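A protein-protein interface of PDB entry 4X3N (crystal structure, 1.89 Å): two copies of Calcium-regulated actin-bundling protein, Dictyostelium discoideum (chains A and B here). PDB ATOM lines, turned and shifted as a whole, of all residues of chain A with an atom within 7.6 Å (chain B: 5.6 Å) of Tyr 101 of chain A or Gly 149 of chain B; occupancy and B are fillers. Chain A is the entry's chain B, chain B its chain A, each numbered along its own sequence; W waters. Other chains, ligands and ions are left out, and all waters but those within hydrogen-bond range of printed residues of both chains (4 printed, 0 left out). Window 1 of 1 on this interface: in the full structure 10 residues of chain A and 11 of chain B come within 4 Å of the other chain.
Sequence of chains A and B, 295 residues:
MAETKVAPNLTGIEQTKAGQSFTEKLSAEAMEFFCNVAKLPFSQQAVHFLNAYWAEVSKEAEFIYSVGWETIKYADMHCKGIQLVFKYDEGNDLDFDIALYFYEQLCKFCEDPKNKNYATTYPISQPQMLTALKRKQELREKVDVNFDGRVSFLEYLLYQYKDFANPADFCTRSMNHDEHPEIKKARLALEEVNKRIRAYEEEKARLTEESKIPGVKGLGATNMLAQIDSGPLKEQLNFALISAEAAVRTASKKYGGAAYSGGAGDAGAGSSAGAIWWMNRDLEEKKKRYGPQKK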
ATOM      1  N   THR A  71      27.599  22.373  -9.894  1.00  0.00           N
ATOM      2  CA  THR A  71      26.791  22.857  -8.786  1.00  0.00           C
ATOM      3  C   THR A  71      25.680  23.769  -9.256  1.00  0.00           C
ATOM      4  O   THR A  71      24.602  23.714  -8.688  1.00  0.00           O
ATOM      5  CB  THR A  71      27.637  23.599  -7.726  1.00  0.00           C
ATOM      6  OG1 THR A  71      28.659  22.708  -7.284  1.00  0.00           O
ATOM      7  CG2 THR A  71      26.789  23.952  -6.496  1.00  0.00           C
ATOM      8  N   ALA A  75      21.615  23.089  -8.859  1.00  0.00           N
ATOM      9  CA  ALA A  75      20.706  24.096  -8.285  1.00  0.00           C
ATOM     10  C   ALA A  75      19.500  24.304  -9.192  1.00  0.00           C
ATOM     11  O   ALA A  75      18.354  24.351  -8.732  1.00  0.00           O
ATOM     12  CB  ALA A  75      21.408  25.422  -8.035  1.00  0.00           C
ATOM     13  N   HIS A  78      17.188  21.131  -9.264  1.00  0.00           N
ATOM     14  CA  HIS A  78      16.260  21.123  -8.153  1.00  0.00           C
ATOM     15  C   HIS A  78      15.124  22.129  -8.327  1.00  0.00           C
ATOM     16  O   HIS A  78      14.004  21.850  -7.975  1.00  0.00           O
ATOM     17  CB  HIS A  78      17.014  21.363  -6.832  1.00  0.00           C
ATOM     18  CG  HIS A  78      18.066  20.341  -6.570  1.00  0.00           C
ATOM     19  ND1 HIS A  78      19.127  20.552  -5.704  1.00  0.00           N
ATOM     20  CD2 HIS A  78      18.261  19.118  -7.127  1.00  0.00           C
ATOM     21  CE1 HIS A  78      19.903  19.478  -5.702  1.00  0.00           C
ATOM     22  NE2 HIS A  78      19.421  18.608  -6.582  1.00  0.00           N
ATOM     23  N   CYS A  79      15.428  23.304  -8.875  1.00  0.00           N
ATOM     24  CA  CYS A  79      14.452  24.381  -8.993  1.00  0.00           C
ATOM     25  C   CYS A  79      13.410  23.838  -9.949  1.00  0.00           C
ATOM     26  O   CYS A  79      12.258  24.075  -9.789  1.00  0.00           O
ATOM     27  CB  CYS A  79      15.105  25.641  -9.589  1.00  0.00           C
ATOM     28  SG  CYS A  79      14.004  26.835 -10.366  1.00  0.00           S
ATOM     29  N   LEU A  94      19.427  31.667 -12.535  1.00  0.00           N
ATOM     30  CA  LEU A  94      18.709  31.318 -11.311  1.00  0.00           C
ATOM     31  C   LEU A  94      18.172  32.581 -10.682  1.00  0.00           C
ATOM     32  O   LEU A  94      18.843  33.628 -10.787  1.00  0.00           O
ATOM     33  CB  LEU A  94      19.677  30.793 -10.295  1.00  0.00           C
ATOM     34  CG  LEU A  94      20.630  29.739 -10.809  1.00  0.00           C
ATOM     35  CD1 LEU A  94      21.676  29.462  -9.716  1.00  0.00           C
ATOM     36  CD2 LEU A  94      19.821  28.539 -11.269  1.00  0.00           C
ATOM     37  N   ASP A  95      17.019  32.508 -10.037  1.00  0.00           N
ATOM     38  CA  ASP A  95      16.574  33.643  -9.207  1.00  0.00           C
ATOM     39  C   ASP A  95      17.446  33.756  -7.960  1.00  0.00           C
ATOM     40  O   ASP A  95      18.247  32.933  -7.737  1.00  0.00           O
ATOM     41  CB  ASP A  95      15.080  33.638  -8.917  1.00  0.00           C
ATOM     42  CG  ASP A  95      14.627  32.576  -7.923  1.00  0.00           C
ATOM     43  OD1 ASP A  95      15.371  32.111  -7.073  1.00  0.00           O
ATOM     44  OD2 ASP A  95      13.425  32.255  -7.962  1.00  0.00           O
ATOM     45  N   PHE A  96      17.251  34.780  -7.156  1.00  0.00           N
ATOM     46  CA  PHE A  96      18.111  34.997  -5.989  1.00  0.00           C
ATOM     47  C   PHE A  96      17.989  33.907  -4.928  1.00  0.00           C
ATOM     48  O   PHE A  96      19.003  33.612  -4.265  1.00  0.00           O
ATOM     49  CB  PHE A  96      17.865  36.381  -5.365  1.00  0.00           C
ATOM     50  CG  PHE A  96      18.383  37.553  -6.201  1.00  0.00           C
ATOM     51  CD1 PHE A  96      19.177  37.369  -7.318  1.00  0.00           C
ATOM     52  CD2 PHE A  96      18.065  38.837  -5.835  1.00  0.00           C
ATOM     53  CE1 PHE A  96      19.671  38.434  -8.043  1.00  0.00           C
ATOM     54  CE2 PHE A  96      18.520  39.904  -6.563  1.00  0.00           C
ATOM     55  CZ  PHE A  96      19.344  39.716  -7.666  1.00  0.00           C
ATOM     56  N   ASP A  97      16.795  33.317  -4.749  1.00  0.00           N
ATOM     57  CA  ASP A  97      16.669  32.210  -3.793  1.00  0.00           C
ATOM     58  C   ASP A  97      17.413  30.993  -4.259  1.00  0.00           C
ATOM     59  O   ASP A  97      18.157  30.413  -3.517  1.00  0.00           O
ATOM     60  CB  ASP A  97      15.209  31.874  -3.467  1.00  0.00           C
ATOM     61  CG  ASP A  97      14.555  32.921  -2.626  1.00  0.00           C
ATOM     62  OD1 ASP A  97      15.228  33.500  -1.742  1.00  0.00           O
ATOM     63  OD2 ASP A  97      13.361  33.167  -2.815  1.00  0.00           O
ATOM     64  N   ILE A  98      17.269  30.617  -5.529  1.00  0.00           N
ATOM     65  CA  ILE A  98      18.057  29.518  -6.065  1.00  0.00           C
ATOM     66  C   ILE A  98      19.572  29.840  -6.105  1.00  0.00           C
ATOM     67  O   ILE A  98      20.421  28.976  -5.798  1.00  0.00           O
ATOM     68  CB  ILE A  98      17.476  29.044  -7.451  1.00  0.00           C
ATOM     69  CG1 ILE A  98      15.942  28.741  -7.349  1.00  0.00           C
ATOM     70  CG2 ILE A  98      18.201  27.824  -7.976  1.00  0.00           C
ATOM     71  CD1 ILE A  98      15.541  27.847  -6.153  1.00  0.00           C
ATOM     72  N   ALA A  99      19.912  31.088  -6.365  1.00  0.00           N
ATOM     73  CA  ALA A  99      21.296  31.495  -6.367  1.00  0.00           C
ATOM     74  C   ALA A  99      21.937  31.309  -5.026  1.00  0.00           C
ATOM     75  O   ALA A  99      23.078  30.858  -4.893  1.00  0.00           O
ATOM     76  CB  ALA A  99      21.406  32.938  -6.761  1.00  0.00           C
ATOM     77  N   LEU A 100      21.168  31.570  -4.023  1.00  0.00           N
ATOM     78  CA  LEU A 100      21.664  31.381  -2.696  1.00  0.00           C
ATOM     79  C   LEU A 100      21.927  29.919  -2.411  1.00  0.00           C
ATOM     80  O   LEU A 100      22.948  29.583  -1.822  1.00  0.00           O
ATOM     81  CB  LEU A 100      20.635  31.956  -1.776  1.00  0.00           C
ATOM     82  CG  LEU A 100      21.102  32.238  -0.406  1.00  0.00           C
ATOM     83  CD1 LEU A 100      20.263  33.357   0.209  1.00  0.00           C
ATOM     84  CD2 LEU A 100      20.910  30.960   0.369  1.00  0.00           C
ATOM     85  N   TYR A 101      21.036  29.025  -2.841  1.00  0.00           N
ATOM     86  CA  TYR A 101      21.278  27.618  -2.652  1.00  0.00           C
ATOM     87  C   TYR A 101      22.541  27.184  -3.414  1.00  0.00           C
ATOM     88  O   TYR A 101      23.303  26.349  -2.899  1.00  0.00           O
ATOM     89  CB  TYR A 101      20.115  26.755  -3.143  1.00  0.00           C
ATOM     90  CG  TYR A 101      18.833  26.747  -2.346  1.00  0.00           C
ATOM     91  CD1 TYR A 101      18.847  26.707  -0.925  1.00  0.00           C
ATOM     92  CD2 TYR A 101      17.607  26.649  -2.981  1.00  0.00           C
ATOM     93  CE1 TYR A 101      17.676  26.632  -0.203  1.00  0.00           C
ATOM     94  CE2 TYR A 101      16.412  26.601  -2.249  1.00  0.00           C
ATOM     95  CZ  TYR A 101      16.464  26.580  -0.857  1.00  0.00           C
ATOM     96  OH  TYR A 101      15.329  26.490  -0.059  1.00  0.00           O
ATOM     97  N   PHE A 102      22.741  27.730  -4.617  1.00  0.00           N
ATOM     98  CA  PHE A 102      23.921  27.461  -5.414  1.00  0.00           C
ATOM     99  C   PHE A 102      25.225  27.844  -4.653  1.00  0.00           C
ATOM    100  O   PHE A 102      26.094  26.988  -4.442  1.00  0.00           O
ATOM    101  CB  PHE A 102      23.818  28.197  -6.766  1.00  0.00           C
ATOM    102  CG  PHE A 102      25.135  28.440  -7.461  1.00  0.00           C
ATOM    103  CD1 PHE A 102      25.867  27.407  -7.979  1.00  0.00           C
ATOM    104  CD2 PHE A 102      25.585  29.680  -7.627  1.00  0.00           C
ATOM    105  CE1 PHE A 102      27.089  27.652  -8.634  1.00  0.00           C
ATOM    106  CE2 PHE A 102      26.808  29.953  -8.244  1.00  0.00           C
ATOM    107  CZ  PHE A 102      27.549  28.923  -8.762  1.00  0.00           C
ATOM    108  N   TYR A 103      25.314  29.097  -4.216  1.00  0.00           N
ATOM    109  CA  TYR A 103      26.493  29.586  -3.508  1.00  0.00           C
ATOM    110  C   TYR A 103      26.700  28.826  -2.227  1.00  0.00           C
ATOM    111  O   TYR A 103      27.838  28.501  -1.889  1.00  0.00           O
ATOM    112  CB  TYR A 103      26.411  31.063  -3.201  1.00  0.00           C
ATOM    113  CG  TYR A 103      26.816  31.943  -4.343  1.00  0.00           C
ATOM    114  CD1 TYR A 103      28.159  32.239  -4.588  1.00  0.00           C
ATOM    115  CD2 TYR A 103      25.858  32.519  -5.178  1.00  0.00           C
ATOM    116  CE1 TYR A 103      28.539  33.060  -5.660  1.00  0.00           C
ATOM    117  CE2 TYR A 103      26.240  33.328  -6.259  1.00  0.00           C
ATOM    118  CZ  TYR A 103      27.590  33.613  -6.481  1.00  0.00           C
ATOM    119  OH  TYR A 103      27.919  34.451  -7.519  1.00  0.00           O
ATOM    120  N   GLU A 104      25.620  28.535  -1.498  1.00  0.00           N
ATOM    121  CA  GLU A 104      25.740  27.725  -0.267  1.00  0.00           C
ATOM    122  C   GLU A 104      26.213  26.333  -0.505  1.00  0.00           C
ATOM    123  O   GLU A 104      27.006  25.834   0.265  1.00  0.00           O
ATOM    124  CB  GLU A 104      24.456  27.712   0.512  1.00  0.00           C
ATOM    125  CG  GLU A 104      24.255  29.129   0.978  1.00  0.00           C
ATOM    126  CD  GLU A 104      23.260  29.301   2.075  1.00  0.00           C
ATOM    127  OE1 GLU A 104      22.594  28.300   2.438  1.00  0.00           O
ATOM    128  OE2 GLU A 104      23.160  30.475   2.517  1.00  0.00           O
ATOM    129  N   GLN A 105      25.750  25.710  -1.589  1.00  0.00           N
ATOM    130  CA  GLN A 105      26.215  24.389  -1.906  1.00  0.00           C
ATOM    131  C   GLN A 105      27.684  24.372  -2.349  1.00  0.00           C
ATOM    132  O   GLN A 105      28.386  23.386  -2.104  1.00  0.00           O
ATOM    133  CB  GLN A 105      25.313  23.708  -2.919  1.00  0.00           C
ATOM    134  CG  GLN A 105      25.852  22.378  -3.425  1.00  0.00           C
ATOM    135  CD  GLN A 105      26.121  21.365  -2.302  1.00  0.00           C
ATOM    136  OE1 GLN A 105      25.480  21.398  -1.230  1.00  0.00           O
ATOM    137  NE2 GLN A 105      27.059  20.458  -2.554  1.00  0.00           N
ATOM    138  N   LEU A 106      28.141  25.425  -3.016  1.00  0.00           N
ATOM    139  CA  LEU A 106      29.543  25.541  -3.311  1.00  0.00           C
ATOM    140  C   LEU A 106      30.398  25.551  -2.064  1.00  0.00           C
ATOM    141  O   LEU A 106      31.414  24.834  -2.017  1.00  0.00           O
ATOM    142  CB  LEU A 106      29.846  26.823  -4.017  1.00  0.00           C
ATOM    143  CG  LEU A 106      29.621  26.829  -5.509  1.00  0.00           C
ATOM    144  CD1 LEU A 106      30.122  28.182  -5.972  1.00  0.00           C
ATOM    145  CD2 LEU A 106      30.338  25.717  -6.234  1.00  0.00           C
ATOM    146  N   CYS A 107      30.030  26.418  -1.138  1.00  0.00           N
ATOM    147  CA  CYS A 107      30.724  26.533   0.157  1.00  0.00           C
ATOM    148  C   CYS A 107      30.710  25.208   0.835  1.00  0.00           C
ATOM    149  O   CYS A 107      31.761  24.716   1.235  1.00  0.00           O
ATOM    150  CB  CYS A 107      30.109  27.632   1.049  1.00  0.00           C
ATOM    151  SG  CYS A 107      30.267  29.277   0.300  1.00  0.00           S
ATOM    152  N   LYS A 108      29.553  24.559   0.890  1.00  0.00           N
ATOM    153  CA  LYS A 108      29.460  23.293   1.587  1.00  0.00           C
ATOM    154  C   LYS A 108      30.393  22.237   1.011  1.00  0.00           C
ATOM    155  O   LYS A 108      31.076  21.505   1.744  1.00  0.00           O
ATOM    156  CB  LYS A 108      28.043  22.780   1.571  1.00  0.00           C
ATOM    157  CG  LYS A 108      27.937  21.344   2.048  1.00  0.00           C
ATOM    158  CD  LYS A 108      26.570  20.790   1.703  1.00  0.00           C
ATOM    159  CE  LYS A 108      25.499  21.323   2.634  1.00  0.00           C
ATOM    160  NZ  LYS A 108      25.255  20.296   3.677  1.00  0.00           N
ATOM    161  N   ARG A 135      24.625  37.691   1.353  1.00  0.00           N
ATOM    162  CA  ARG A 135      24.599  37.156   0.008  1.00  0.00           C
ATOM    163  C   ARG A 135      23.689  37.914  -0.980  1.00  0.00           C
ATOM    164  O   ARG A 135      24.139  38.373  -2.062  1.00  0.00           O
ATOM    165  CB  ARG A 135      24.264  35.692   0.076  1.00  0.00           C
ATOM    166  CG  ARG A 135      24.401  34.970  -1.254  1.00  0.00           C
ATOM    167  CD  ARG A 135      25.301  33.770  -1.028  1.00  0.00           C
ATOM    168  NE  ARG A 135      26.572  34.142  -1.544  1.00  0.00           N
ATOM    169  CZ  ARG A 135      27.745  33.630  -1.183  1.00  0.00           C
ATOM    170  NH1 ARG A 135      27.848  32.688  -0.242  1.00  0.00           N
ATOM    171  NH2 ARG A 135      28.813  34.101  -1.823  1.00  0.00           N
ATOM    172  N   LEU A 139      24.511  39.833  -4.403  1.00  0.00           N
ATOM    173  CA  LEU A 139      23.895  39.580  -5.705  1.00  0.00           C
ATOM    174  C   LEU A 139      23.326  40.826  -6.307  1.00  0.00           C
ATOM    175  O   LEU A 139      23.530  41.059  -7.513  1.00  0.00           O
ATOM    176  CB  LEU A 139      22.849  38.467  -5.650  1.00  0.00           C
ATOM    177  CG  LEU A 139      23.236  37.156  -4.988  1.00  0.00           C
ATOM    178  CD1 LEU A 139      22.028  36.250  -4.843  1.00  0.00           C
ATOM    179  CD2 LEU A 139      24.371  36.475  -5.719  1.00  0.00           C
ATOM    180  N   LEU B  94       3.978  27.533  -3.213  1.00  0.00           N
ATOM    181  CA  LEU B  94       4.110  28.960  -3.064  1.00  0.00           C
ATOM    182  C   LEU B  94       5.602  29.381  -3.133  1.00  0.00           C
ATOM    183  O   LEU B  94       6.501  28.701  -2.582  1.00  0.00           O
ATOM    184  CB  LEU B  94       3.584  29.402  -1.692  1.00  0.00           C
ATOM    185  CG  LEU B  94       2.236  28.837  -1.175  1.00  0.00           C
ATOM    186  CD1 LEU B  94       1.944  29.433   0.210  1.00  0.00           C
ATOM    187  CD2 LEU B  94       1.127  29.169  -2.171  1.00  0.00           C
ATOM    188  N   ASP B  95       5.878  30.538  -3.743  1.00  0.00           N
ATOM    189  CA  ASP B  95       7.229  31.070  -3.667  1.00  0.00           C
ATOM    190  C   ASP B  95       7.425  31.553  -2.229  1.00  0.00           C
ATOM    191  O   ASP B  95       6.440  31.592  -1.454  1.00  0.00           O
ATOM    192  CB  ASP B  95       7.502  32.092  -4.764  1.00  0.00           C
ATOM    193  CG  ASP B  95       6.857  33.481  -4.565  1.00  0.00           C
ATOM    194  OD1 ASP B  95       6.556  33.974  -3.435  1.00  0.00           O
ATOM    195  OD2 ASP B  95       6.746  34.168  -5.649  1.00  0.00           O
ATOM    196  N   PHE B  96       8.618  31.978  -1.883  1.00  0.00           N
ATOM    197  CA  PHE B  96       8.889  32.340  -0.497  1.00  0.00           C
ATOM    198  C   PHE B  96       8.147  33.625  -0.009  1.00  0.00           C
ATOM    199  O   PHE B  96       7.779  33.760   1.202  1.00  0.00           O
ATOM    200  CB  PHE B  96      10.407  32.483  -0.266  1.00  0.00           C
ATOM    201  CG  PHE B  96      11.179  31.190  -0.175  1.00  0.00           C
ATOM    202  CD1 PHE B  96      10.604  29.960  -0.344  1.00  0.00           C
ATOM    203  CD2 PHE B  96      12.546  31.256   0.023  1.00  0.00           C
ATOM    204  CE1 PHE B  96      11.365  28.821  -0.293  1.00  0.00           C
ATOM    205  CE2 PHE B  96      13.310  30.117   0.091  1.00  0.00           C
ATOM    206  CZ  PHE B  96      12.721  28.888  -0.057  1.00  0.00           C
ATOM    207  N   LEU B 139      12.429  28.699   5.950  1.00  0.00           N
ATOM    208  CA  LEU B 139      11.959  28.062   4.693  1.00  0.00           C
ATOM    209  C   LEU B 139      13.123  27.396   3.995  1.00  0.00           C
ATOM    210  O   LEU B 139      13.057  26.267   3.569  1.00  0.00           O
ATOM    211  CB  LEU B 139      11.324  29.117   3.746  1.00  0.00           C
ATOM    212  CG  LEU B 139      10.079  29.839   4.266  1.00  0.00           C
ATOM    213  CD1 LEU B 139       9.452  30.660   3.161  1.00  0.00           C
ATOM    214  CD2 LEU B 139       9.048  28.894   4.839  1.00  0.00           C
ATOM    215  N   ARG B 140      14.195  28.162   3.879  1.00  0.00           N
ATOM    216  CA  ARG B 140      15.427  27.816   3.229  1.00  0.00           C
ATOM    217  C   ARG B 140      16.223  26.722   3.935  1.00  0.00           C
ATOM    218  O   ARG B 140      16.749  25.841   3.284  1.00  0.00           O
ATOM    219  CB  ARG B 140      16.271  29.106   3.218  1.00  0.00           C
ATOM    220  CG  ARG B 140      17.479  29.117   2.385  1.00  0.00           C
ATOM    221  CD  ARG B 140      18.038  30.525   2.440  1.00  0.00           C
ATOM    222  NE  ARG B 140      17.257  31.416   1.579  1.00  0.00           N
ATOM    223  CZ  ARG B 140      16.797  32.604   1.948  1.00  0.00           C
ATOM    224  NH1 ARG B 140      17.051  33.086   3.177  1.00  0.00           N
ATOM    225  NH2 ARG B 140      16.129  33.328   1.046  1.00  0.00           N
ATOM    226  N   GLU B 141      16.284  26.776   5.267  1.00  0.00           N
ATOM    227  CA  GLU B 141      17.015  25.782   6.042  1.00  0.00           C
ATOM    228  C   GLU B 141      16.232  24.504   6.297  1.00  0.00           C
ATOM    229  O   GLU B 141      16.799  23.441   6.331  1.00  0.00           O
ATOM    230  CB  GLU B 141      17.393  26.374   7.405  1.00  0.00           C
ATOM    231  CG  GLU B 141      18.610  27.275   7.281  1.00  0.00           C
ATOM    232  CD  GLU B 141      19.043  27.908   8.594  1.00  0.00           C
ATOM    233  OE1 GLU B 141      19.712  28.953   8.545  1.00  0.00           O
ATOM    234  OE2 GLU B 141      18.680  27.370   9.646  1.00  0.00           O
ATOM    235  N   ASP B 144      11.871  23.972   2.836  1.00  0.00           N
ATOM    236  CA  ASP B 144      12.062  23.666   1.395  1.00  0.00           C
ATOM    237  C   ASP B 144      13.036  22.526   1.128  1.00  0.00           C
ATOM    238  O   ASP B 144      14.184  22.744   0.611  1.00  0.00           O
ATOM    239  CB  ASP B 144      12.478  24.925   0.636  1.00  0.00           C
ATOM    240  CG  ASP B 144      12.619  24.695  -0.870  1.00  0.00           C
ATOM    241  OD1 ASP B 144      12.000  23.762  -1.404  1.00  0.00           O
ATOM    242  OD2 ASP B 144      13.349  25.481  -1.494  1.00  0.00           O
ATOM    243  N   PHE B 147      14.634  21.924  -2.366  1.00  0.00           N
ATOM    244  CA  PHE B 147      15.438  23.052  -2.843  1.00  0.00           C
ATOM    245  C   PHE B 147      14.963  23.717  -4.123  1.00  0.00           C
ATOM    246  O   PHE B 147      15.786  24.065  -4.999  1.00  0.00           O
ATOM    247  CB  PHE B 147      16.907  22.638  -2.940  1.00  0.00           C
ATOM    248  CG  PHE B 147      17.490  22.228  -1.617  1.00  0.00           C
ATOM    249  CD1 PHE B 147      17.481  20.935  -1.235  1.00  0.00           C
ATOM    250  CD2 PHE B 147      18.039  23.157  -0.776  1.00  0.00           C
ATOM    251  CE1 PHE B 147      18.021  20.551  -0.013  1.00  0.00           C
ATOM    252  CE2 PHE B 147      18.573  22.791   0.448  1.00  0.00           C
ATOM    253  CZ  PHE B 147      18.556  21.474   0.822  1.00  0.00           C
ATOM    254  N   ASP B 148      13.632  23.908  -4.229  1.00  0.00           N
ATOM    255  CA  ASP B 148      13.097  24.501  -5.435  1.00  0.00           C
ATOM    256  C   ASP B 148      12.675  25.920  -5.244  1.00  0.00           C
ATOM    257  O   ASP B 148      12.145  26.509  -6.146  1.00  0.00           O
ATOM    258  CB  ASP B 148      12.014  23.600  -6.088  1.00  0.00           C
ATOM    259  CG  ASP B 148      10.755  23.501  -5.253  1.00  0.00           C
ATOM    260  OD1 ASP B 148      10.754  24.061  -4.176  1.00  0.00           O
ATOM    261  OD2 ASP B 148       9.779  22.873  -5.674  1.00  0.00           O
ATOM    262  N   GLY B 149      12.926  26.480  -4.060  1.00  0.00           N
ATOM    263  CA  GLY B 149      12.457  27.805  -3.671  1.00  0.00           C
ATOM    264  C   GLY B 149      10.930  27.918  -3.541  1.00  0.00           C
ATOM    265  O   GLY B 149      10.385  29.036  -3.563  1.00  0.00           O
ATOM    266  N   ARG B 150      10.236  26.773  -3.462  1.00  0.00           N
ATOM    267  CA  ARG B 150       8.794  26.738  -3.327  1.00  0.00           C
ATOM    268  C   ARG B 150       8.386  25.967  -2.052  1.00  0.00           C
ATOM    269  O   ARG B 150       9.100  25.041  -1.588  1.00  0.00           O
ATOM    270  CB  ARG B 150       8.161  26.054  -4.526  1.00  0.00           C
ATOM    271  CG  ARG B 150       8.611  26.473  -5.927  1.00  0.00           C
ATOM    272  CD  ARG B 150       8.112  27.823  -6.372  1.00  0.00           C
ATOM    273  NE  ARG B 150       6.654  27.883  -6.457  1.00  0.00           N
ATOM    274  CZ  ARG B 150       5.979  28.924  -6.919  1.00  0.00           C
ATOM    275  NH1 ARG B 150       6.640  30.005  -7.381  1.00  0.00           N
ATOM    276  NH2 ARG B 150       4.645  28.907  -6.932  1.00  0.00           N
ATOM    277  N   VAL B 151       7.268  26.370  -1.470  1.00  0.00           N
ATOM    278  CA  VAL B 151       6.687  25.683  -0.334  1.00  0.00           C
ATOM    279  C   VAL B 151       5.336  25.047  -0.732  1.00  0.00           C
ATOM    280  O   VAL B 151       4.406  25.749  -1.158  1.00  0.00           O
ATOM    281  CB  VAL B 151       6.501  26.612   0.865  1.00  0.00           C
ATOM    282  CG1 VAL B 151       5.848  25.872   1.991  1.00  0.00           C
ATOM    283  CG2 VAL B 151       7.827  27.185   1.335  1.00  0.00           C
HETATM  284  O   HOH W   1      17.238  29.859  -1.043  1.00  0.00           O
HETATM  285  O   HOH W   2      11.126  31.754  -3.655  1.00  0.00           O
HETATM  286  O   HOH W   3      11.519  28.187  -7.972  1.00  0.00           O
HETATM  287  O   HOH W   4      18.150  24.600  -5.980  1.00  0.00           O
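NH2 of Arg 140 of chain B lies within salt-bridge range of OD1 of Asp 97 of chain A (2.9 Å).
The side-chain carboxylate (OD2) of Asp 144 of chain B lies within hydrogen-bond range of the side-chain hydroxyl (OH) of Tyr 101 of chain A (2.6 Å).
Water W3 bridges O of Asp 148 of chain B (2.6 Å) and SG of Cys 79 of chain A (3.7 Å).
Water W4 lies within hydrogen-bond range of O of Phe 147 of chain B (2.6 Å) and O of Ala 75 of chain A (2.8 Å).
Water W1 bridges the backbone carbonyl oxygen (O) of Asp 97 of chain A (2.7 Å) and the guanidinium group (NE) of Arg 140 of chain B (3.0 Å).
Water W2 lies within hydrogen-bond range of OD2 of Asp 97 of chain A, O of Gly 149 of chain B and N of Phe 96 of chain B.
Positions printed for both chains: 94, 95, 96 and 139.
The backbone NH (N) of Asp 144 of chain B is in hydrogen-bond range of the backbone carbonyl oxygen (O) of Leu 139 of chain B (2.7 Å).
OD1 of Asp 144 of chain B lies close to N of Phe 147 of chain B (3.4 Å).
The side-chain carboxylate (OD2) of Asp 144 of chain B sits at hydrogen-bond distance from the backbone NH (N) of Gly 149 of chain B (2.8 Å).
The side-chain carboxylate (OD1) of Asp 95 of chain A sits at hydrogen-bond distance from the backbone NH (N) of Asp 97 of chain A, at 3.0 Å.
The backbone NH (N) of Ile 98 of chain A sits at hydrogen-bond distance from the side-chain carboxylate (OD1) of Asp 95 of chain A.
Of the printed residues of chain B, Cys 79 of chain A touches Phe 147 (3.97 Å) and Asp 148 (3.7 Å).
Asp 95 of chain A touches none of the printed residues of chain B.
Of the printed residues of chain B, Asp 97 of chain A touches Phe 96 (3.5 Å) and Arg 140 (2.9 Å).
Tyr 101 of chain A touches five residues of chain B.
Of the printed residues of chain A, Phe 96 of chain B touches Asp 97 (3.5 Å) and Tyr 101 (3.5 Å).
Printed residues of chain A within 4 Å of Arg 140 of chain B: Asp 97, Leu 100 and Tyr 101.
Printed residues of chain A within 4 Å of Phe 147 of chain B: His 78, Cys 79, Ile 98 and Tyr 101.
Gly 149 of chain B touches just these residues of chain A: Ile 98 (3.6 Å) and Tyr 101 (3.9 Å).
The nearest residue of chain A that does not touch Gly 149 of chain B is Asp 97 of chain A (4.9 Å).
Among the printed residues, pairs that only touch across the chains: His 78 of chain A with Phe 147 of chain B, His 78 of chain A with Asp 148 of chain B, Cys 79 of chain A with Phe 147 of chain B, Cys 79 of chain A with Asp 148 of chain B, Asp 97 of chain A with Phe 96 of chain B, Ile 98 of chain A with Phe 147 of chain B, Ile 98 of chain A with Asp 148 of chain B, Ile 98 of chain A with Gly 149 of chain B, Leu 100 of chain A with Arg 140 of chain B, Tyr 101 of chain A with Phe 96 of chain B, Tyr 101 of chain A with Arg 140 of chain B, Tyr 101 of chain A with Phe 147 of chain B and Tyr 101 of chain A with Gly 149 of chain B.
Of the 21 printed residues of chain A, 6 touch a printed residue of chain B.
Hydrophobic or aromatic side chains of chain A within 4 Å of the printed part of chain B: His 78, Ile 98, Leu 100 and Tyr 101.
Of the 12 printed residues of chain B, 6 touch a printed residue of chain A.
Hydrophobic or aromatic side chains of chain B that line the printed part of chain A: Phe 96 and Phe 147.
Among the printed residues, Asp or Glu carboxylates within 4 Å of a Lys or Arg side-chain nitrogen of the other chain: Asp 97 of chain A with Arg 140 of chain B.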
